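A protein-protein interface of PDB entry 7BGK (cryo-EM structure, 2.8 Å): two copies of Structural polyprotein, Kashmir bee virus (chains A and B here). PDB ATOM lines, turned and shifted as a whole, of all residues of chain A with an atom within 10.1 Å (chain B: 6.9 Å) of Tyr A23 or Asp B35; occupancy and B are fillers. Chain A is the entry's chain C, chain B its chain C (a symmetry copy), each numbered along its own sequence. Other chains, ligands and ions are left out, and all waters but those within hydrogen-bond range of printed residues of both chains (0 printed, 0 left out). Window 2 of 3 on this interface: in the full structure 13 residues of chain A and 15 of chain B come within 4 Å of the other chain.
Among the printed residues, pairs that only touch across the chains: Lys A24 with Pro B36, Leu A22 with Ala B33, Tyr A23 with Asp B35, Leu A22 with Pro B31, Leu A22 with Tyr B34, Ser A21 with Ala B33 and Leu A22 with Pro B36.
Gly A19 touches none of the printed residues of chain B.
Of the printed residues of chain B, Ser A21 touches Ala B33.
Of the printed residues of chain B, Leu A22 touches Pro B31, Ala B33, Tyr B34 and Pro B36.
Of chain B, only Tyr B34 (3.0 Å) and Asp B35 (3.5 Å) come within 4 Å of Tyr A23.
Ile A26 touches none of the printed residues of chain B.
Of the printed residues of chain A, Pro B31 touches Leu A22.
Ala B33 touches just these residues of chain A: Ser A21 and Leu A22.
Tyr B34 touches two residues of chain A.
Of chain A, only Leu A22 (3.8 Å) and Lys A24 (3.0 Å) come within 4 Å of Pro B36.
Asn B37 touches none of the printed residues of chain A.
No residue of chain A comes within 4 Å of Asn B38.
The nearest residue of chain B that does not touch Tyr A23 is Pro B36 (4.5 Å).
The nearest printed residue of chain A that does not touch Pro B31 is Trp A18 (4.1 Å).
No position is printed for both chains.
The side-chain hydroxyl (OH) of Tyr A23 lies close to the side-chain amino group (NZ) of Lys A24 (3.3 Å).
The backbone NH (N) of Asn B37 lies within hydrogen-bond range of the side-chain carboxylate (OD1) of Asp B35 (3.0 Å).
The backbone NH (N) of Tyr A23 sits close to the backbone carbonyl oxygen (O) of Tyr B34, at 3.1 Å.
Of the 8 printed residues of chain B, 5 touch a printed residue of chain A.
Hydrophobic or aromatic side chains of chain B within 4 Å of the printed part of chain A: Tyr B34 and Pro B36.
Among the printed residues, no Asp or Glu carboxylate lies within 4 Å of a Lys or Arg side-chain nitrogen of the other chain.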
ATOM      1  N   TRP A  18     -28.733 -20.394  15.120  1.00  0.00           N
ATOM      2  CA  TRP A  18     -29.527 -20.375  13.899  1.00  0.00           C
ATOM      3  C   TRP A  18     -28.975 -19.298  12.977  1.00  0.00           C
ATOM      4  O   TRP A  18     -29.104 -18.103  13.257  1.00  0.00           O
ATOM      5  CB  TRP A  18     -30.994 -20.114  14.219  1.00  0.00           C
ATOM      6  CG  TRP A  18     -31.937 -20.419  13.102  1.00  0.00           C
ATOM      7  CD1 TRP A  18     -32.742 -21.503  12.995  1.00  0.00           C
ATOM      8  CD2 TRP A  18     -32.181 -19.624  11.937  1.00  0.00           C
ATOM      9  NE1 TRP A  18     -33.472 -21.442  11.841  1.00  0.00           N
ATOM     10  CE2 TRP A  18     -33.148 -20.294  11.171  1.00  0.00           C
ATOM     11  CE3 TRP A  18     -31.676 -18.412  11.466  1.00  0.00           C
ATOM     12  CZ2 TRP A  18     -33.612 -19.800   9.962  1.00  0.00           C
ATOM     13  CZ3 TRP A  18     -32.141 -17.926  10.273  1.00  0.00           C
ATOM     14  CH2 TRP A  18     -33.097 -18.615   9.533  1.00  0.00           C
ATOM     15  N   GLY A  19     -28.360 -19.718  11.878  1.00  0.00           N
ATOM     16  CA  GLY A  19     -27.820 -18.772  10.929  1.00  0.00           C
ATOM     17  C   GLY A  19     -26.503 -18.160  11.325  1.00  0.00           C
ATOM     18  O   GLY A  19     -26.204 -17.038  10.910  1.00  0.00           O
ATOM     19  N   TYR A  20     -25.701 -18.862  12.123  1.00  0.00           N
ATOM     20  CA  TYR A  20     -24.404 -18.335  12.514  1.00  0.00           C
ATOM     21  C   TYR A  20     -23.458 -18.188  11.334  1.00  0.00           C
ATOM     22  O   TYR A  20     -22.497 -17.418  11.418  1.00  0.00           O
ATOM     23  CB  TYR A  20     -23.792 -19.232  13.588  1.00  0.00           C
ATOM     24  CG  TYR A  20     -23.410 -20.618  13.135  1.00  0.00           C
ATOM     25  CD1 TYR A  20     -24.349 -21.629  13.085  1.00  0.00           C
ATOM     26  CD2 TYR A  20     -22.107 -20.926  12.798  1.00  0.00           C
ATOM     27  CE1 TYR A  20     -24.008 -22.895  12.689  1.00  0.00           C
ATOM     28  CE2 TYR A  20     -21.757 -22.191  12.400  1.00  0.00           C
ATOM     29  CZ  TYR A  20     -22.713 -23.172  12.348  1.00  0.00           C
ATOM     30  OH  TYR A  20     -22.369 -24.439  11.955  1.00  0.00           O
ATOM     31  N   SER A  21     -23.719 -18.882  10.236  1.00  0.00           N
ATOM     32  CA  SER A  21     -22.893 -18.805   9.045  1.00  0.00           C
ATOM     33  C   SER A  21     -23.310 -17.687   8.104  1.00  0.00           C
ATOM     34  O   SER A  21     -22.681 -17.509   7.057  1.00  0.00           O
ATOM     35  CB  SER A  21     -22.916 -20.141   8.317  1.00  0.00           C
ATOM     36  OG  SER A  21     -22.061 -21.061   8.960  1.00  0.00           O
ATOM     37  N   LEU A  22     -24.353 -16.945   8.445  1.00  0.00           N
ATOM     38  CA  LEU A  22     -24.793 -15.806   7.664  1.00  0.00           C
ATOM     39  C   LEU A  22     -24.126 -14.535   8.171  1.00  0.00           C
ATOM     40  O   LEU A  22     -23.785 -14.417   9.350  1.00  0.00           O
ATOM     41  CB  LEU A  22     -26.311 -15.667   7.735  1.00  0.00           C
ATOM     42  CG  LEU A  22     -27.120 -16.924   7.439  1.00  0.00           C
ATOM     43  CD1 LEU A  22     -28.551 -16.744   7.860  1.00  0.00           C
ATOM     44  CD2 LEU A  22     -27.058 -17.257   5.989  1.00  0.00           C
ATOM     45  N   TYR A  23     -23.938 -13.580   7.264  1.00  0.00           N
ATOM     46  CA  TYR A  23     -23.271 -12.334   7.604  1.00  0.00           C
ATOM     47  C   TYR A  23     -24.205 -11.305   8.213  1.00  0.00           C
ATOM     48  O   TYR A  23     -23.725 -10.327   8.791  1.00  0.00           O
ATOM     49  CB  TYR A  23     -22.612 -11.746   6.360  1.00  0.00           C
ATOM     50  CG  TYR A  23     -23.479 -10.806   5.560  1.00  0.00           C
ATOM     51  CD1 TYR A  23     -24.460 -11.288   4.721  1.00  0.00           C
ATOM     52  CD2 TYR A  23     -23.294  -9.437   5.619  1.00  0.00           C
ATOM     53  CE1 TYR A  23     -25.242 -10.446   3.985  1.00  0.00           C
ATOM     54  CE2 TYR A  23     -24.075  -8.586   4.884  1.00  0.00           C
ATOM     55  CZ  TYR A  23     -25.046  -9.097   4.064  1.00  0.00           C
ATOM     56  OH  TYR A  23     -25.834  -8.258   3.321  1.00  0.00           O
ATOM     57  N   LYS A  24     -25.511 -11.508   8.107  1.00  0.00           N
ATOM     58  CA  LYS A  24     -26.502 -10.529   8.514  1.00  0.00           C
ATOM     59  C   LYS A  24     -27.462 -11.197   9.479  1.00  0.00           C
ATOM     60  O   LYS A  24     -27.986 -12.277   9.191  1.00  0.00           O
ATOM     61  CB  LYS A  24     -27.241  -9.970   7.299  1.00  0.00           C
ATOM     62  CG  LYS A  24     -28.101  -8.778   7.578  1.00  0.00           C
ATOM     63  CD  LYS A  24     -28.793  -8.303   6.328  1.00  0.00           C
ATOM     64  CE  LYS A  24     -27.958  -7.286   5.607  1.00  0.00           C
ATOM     65  NZ  LYS A  24     -28.624  -6.790   4.386  1.00  0.00           N
ATOM     66  N   GLY A  25     -27.674 -10.570  10.617  1.00  0.00           N
ATOM     67  CA  GLY A  25     -28.566 -11.107  11.622  1.00  0.00           C
ATOM     68  C   GLY A  25     -28.157 -10.645  12.999  1.00  0.00           C
ATOM     69  O   GLY A  25     -27.068 -10.130  13.216  1.00  0.00           O
ATOM     70  N   ILE A  26     -29.063 -10.845  13.943  1.00  0.00           N
ATOM     71  CA  ILE A  26     -28.836 -10.451  15.325  1.00  0.00           C
ATOM     72  C   ILE A  26     -28.121 -11.591  16.036  1.00  0.00           C
ATOM     73  O   ILE A  26     -28.675 -12.683  16.195  1.00  0.00           O
ATOM     74  CB  ILE A  26     -30.158 -10.091  16.017  1.00  0.00           C
ATOM     75  CG1 ILE A  26     -30.773  -8.862  15.348  1.00  0.00           C
ATOM     76  CG2 ILE A  26     -29.933  -9.832  17.474  1.00  0.00           C
ATOM     77  CD1 ILE A  26     -32.191  -8.605  15.707  1.00  0.00           C
ATOM     78  N   ASP A  27     -26.886 -11.336  16.456  1.00  0.00           N
ATOM     79  CA  ASP A  27     -26.052 -12.349  17.077  1.00  0.00           C
ATOM     80  C   ASP A  27     -26.324 -12.443  18.569  1.00  0.00           C
ATOM     81  O   ASP A  27     -26.476 -11.429  19.254  1.00  0.00           O
ATOM     82  CB  ASP A  27     -24.575 -12.043  16.855  1.00  0.00           C
ATOM     83  CG  ASP A  27     -23.724 -13.291  16.795  1.00  0.00           C
ATOM     84  OD1 ASP A  27     -24.097 -14.302  17.424  1.00  0.00           O
ATOM     85  OD2 ASP A  27     -22.677 -13.260  16.119  1.00  0.00           O
ATOM     86  N   VAL A 268     -18.867 -12.904  -7.064  1.00  0.00           N
ATOM     87  CA  VAL A 268     -18.538 -14.216  -6.529  1.00  0.00           C
ATOM     88  C   VAL A 268     -19.797 -14.795  -5.907  1.00  0.00           C
ATOM     89  O   VAL A 268     -20.587 -14.065  -5.298  1.00  0.00           O
ATOM     90  CB  VAL A 268     -17.397 -14.133  -5.502  1.00  0.00           C
ATOM     91  CG1 VAL A 268     -16.082 -13.904  -6.199  1.00  0.00           C
ATOM     92  CG2 VAL A 268     -17.665 -13.023  -4.505  1.00  0.00           C
ATOM     93  N   VAL A 269     -19.987 -16.102  -6.061  1.00  0.00           N
ATOM     94  CA  VAL A 269     -21.317 -16.679  -5.919  1.00  0.00           C
ATOM     95  C   VAL A 269     -21.539 -17.281  -4.539  1.00  0.00           C
ATOM     96  O   VAL A 269     -22.360 -16.774  -3.766  1.00  0.00           O
ATOM     97  CB  VAL A 269     -21.549 -17.711  -7.032  1.00  0.00           C
ATOM     98  CG1 VAL A 269     -22.841 -18.466  -6.850  1.00  0.00           C
ATOM     99  CG2 VAL A 269     -21.578 -17.001  -8.333  1.00  0.00           C
ATOM    100  N   GLU A 270     -20.806 -18.340  -4.200  1.00  0.00           N
ATOM    101  CA  GLU A 270     -21.047 -18.940  -2.898  1.00  0.00           C
ATOM    102  C   GLU A 270     -19.776 -18.957  -2.059  1.00  0.00           C
ATOM    103  O   GLU A 270     -18.675 -19.116  -2.591  1.00  0.00           O
ATOM    104  CB  GLU A 270     -21.622 -20.358  -3.020  1.00  0.00           C
ATOM    105  CG  GLU A 270     -20.663 -21.480  -3.194  1.00  0.00           C
ATOM    106  CD  GLU A 270     -21.358 -22.818  -3.143  1.00  0.00           C
ATOM    107  OE1 GLU A 270     -21.985 -23.198  -4.149  1.00  0.00           O
ATOM    108  OE2 GLU A 270     -21.287 -23.487  -2.095  1.00  0.00           O
ATOM    109  N   PRO A 271     -19.904 -18.800  -0.741  1.00  0.00           N
ATOM    110  CA  PRO A 271     -18.720 -18.593   0.101  1.00  0.00           C
ATOM    111  C   PRO A 271     -17.982 -19.874   0.454  1.00  0.00           C
ATOM    112  O   PRO A 271     -17.215 -19.904   1.419  1.00  0.00           O
ATOM    113  CB  PRO A 271     -19.300 -17.916   1.346  1.00  0.00           C
ATOM    114  CG  PRO A 271     -20.701 -18.311   1.384  1.00  0.00           C
ATOM    115  CD  PRO A 271     -21.154 -18.625   0.017  1.00  0.00           C
ATOM    116  N   PRO B  31     -30.702 -21.346   5.791  1.00  0.00           N
ATOM    117  CA  PRO B  31     -30.066 -21.328   4.475  1.00  0.00           C
ATOM    118  C   PRO B  31     -28.558 -21.431   4.551  1.00  0.00           C
ATOM    119  O   PRO B  31     -27.906 -20.674   5.275  1.00  0.00           O
ATOM    120  CB  PRO B  31     -30.512 -19.983   3.905  1.00  0.00           C
ATOM    121  CG  PRO B  31     -30.669 -19.122   5.084  1.00  0.00           C
ATOM    122  CD  PRO B  31     -30.992 -19.984   6.263  1.00  0.00           C
ATOM    123  N   ALA B  33     -26.018 -20.236   3.105  1.00  0.00           N
ATOM    124  CA  ALA B  33     -25.777 -19.131   2.195  1.00  0.00           C
ATOM    125  C   ALA B  33     -24.996 -18.044   2.919  1.00  0.00           C
ATOM    126  O   ALA B  33     -24.512 -18.234   4.037  1.00  0.00           O
ATOM    127  CB  ALA B  33     -27.103 -18.595   1.648  1.00  0.00           C
ATOM    128  N   TYR B  34     -24.869 -16.899   2.254  1.00  0.00           N
ATOM    129  CA  TYR B  34     -24.220 -15.704   2.770  1.00  0.00           C
ATOM    130  C   TYR B  34     -25.233 -14.709   3.317  1.00  0.00           C
ATOM    131  O   TYR B  34     -25.088 -14.229   4.443  1.00  0.00           O
ATOM    132  CB  TYR B  34     -23.380 -15.088   1.644  1.00  0.00           C
ATOM    133  CG  TYR B  34     -22.944 -13.652   1.792  1.00  0.00           C
ATOM    134  CD1 TYR B  34     -21.840 -13.320   2.553  1.00  0.00           C
ATOM    135  CD2 TYR B  34     -23.591 -12.639   1.108  1.00  0.00           C
ATOM    136  CE1 TYR B  34     -21.424 -12.017   2.663  1.00  0.00           C
ATOM    137  CE2 TYR B  34     -23.183 -11.340   1.211  1.00  0.00           C
ATOM    138  CZ  TYR B  34     -22.097 -11.029   1.988  1.00  0.00           C
ATOM    139  OH  TYR B  34     -21.688  -9.722   2.087  1.00  0.00           O
ATOM    140  N   ASP B  35     -26.286 -14.426   2.553  1.00  0.00           N
ATOM    141  CA  ASP B  35     -27.325 -13.474   2.907  1.00  0.00           C
ATOM    142  C   ASP B  35     -28.551 -14.212   3.409  1.00  0.00           C
ATOM    143  O   ASP B  35     -28.978 -15.182   2.769  1.00  0.00           O
ATOM    144  CB  ASP B  35     -27.697 -12.630   1.690  1.00  0.00           C
ATOM    145  CG  ASP B  35     -28.235 -11.265   2.058  1.00  0.00           C
ATOM    146  OD1 ASP B  35     -28.999 -11.157   3.035  1.00  0.00           O
ATOM    147  OD2 ASP B  35     -27.904 -10.294   1.352  1.00  0.00           O
ATOM    148  N   PRO B  36     -29.150 -13.816   4.537  1.00  0.00           N
ATOM    149  CA  PRO B  36     -30.446 -14.398   4.900  1.00  0.00           C
ATOM    150  C   PRO B  36     -31.552 -13.996   3.955  1.00  0.00           C
ATOM    151  O   PRO B  36     -32.546 -14.722   3.836  1.00  0.00           O
ATOM    152  CB  PRO B  36     -30.698 -13.857   6.311  1.00  0.00           C
ATOM    153  CG  PRO B  36     -29.443 -13.190   6.725  1.00  0.00           C
ATOM    154  CD  PRO B  36     -28.719 -12.809   5.513  1.00  0.00           C
ATOM    155  N   ASN B  37     -31.410 -12.858   3.288  1.00  0.00           N
ATOM    156  CA  ASN B  37     -32.343 -12.398   2.269  1.00  0.00           C
ATOM    157  C   ASN B  37     -31.911 -12.883   0.894  1.00  0.00           C
ATOM    158  O   ASN B  37     -31.777 -12.121  -0.059  1.00  0.00           O
ATOM    159  CB  ASN B  37     -32.438 -10.883   2.318  1.00  0.00           C
ATOM    160  CG  ASN B  37     -33.125 -10.386   3.561  1.00  0.00           C
ATOM    161  OD1 ASN B  37     -32.513  -9.732   4.400  1.00  0.00           O
ATOM    162  ND2 ASN B  37     -34.410 -10.679   3.682  1.00  0.00           N
ATOM    163  N   ASN B  38     -31.685 -14.185   0.805  1.00  0.00           N
ATOM    164  CA  ASN B  38     -31.353 -14.849  -0.447  1.00  0.00           C
ATOM    165  C   ASN B  38     -32.628 -15.102  -1.238  1.00  0.00           C
ATOM    166  O   ASN B  38     -33.447 -15.944  -0.856  1.00  0.00           O
ATOM    167  CB  ASN B  38     -30.606 -16.148  -0.163  1.00  0.00           C
ATOM    168  CG  ASN B  38     -30.225 -16.891  -1.415  1.00  0.00           C
ATOM    169  OD1 ASN B  38     -31.077 -17.427  -2.117  1.00  0.00           O
ATOM    170  ND2 ASN B  38     -28.936 -16.955  -1.688  1.00  0.00           N
ATOM    171  N   GLU B  39     -32.802 -14.371  -2.334  1.00  0.00           N
ATOM    172  CA  GLU B  39     -33.939 -14.543  -3.222  1.00  0.00           C
ATOM    173  C   GLU B  39     -33.407 -14.702  -4.632  1.00  0.00           C
ATOM    174  O   GLU B  39     -32.543 -13.934  -5.062  1.00  0.00           O
ATOM    175  CB  GLU B  39     -34.918 -13.352  -3.238  1.00  0.00           C
ATOM    176  CG  GLU B  39     -35.664 -12.972  -1.977  1.00  0.00           C
ATOM    177  CD  GLU B  39     -34.888 -12.040  -1.060  1.00  0.00           C
ATOM    178  OE1 GLU B  39     -33.789 -11.596  -1.446  1.00  0.00           O
ATOM    179  OE2 GLU B  39     -35.382 -11.748   0.051  1.00  0.00           O
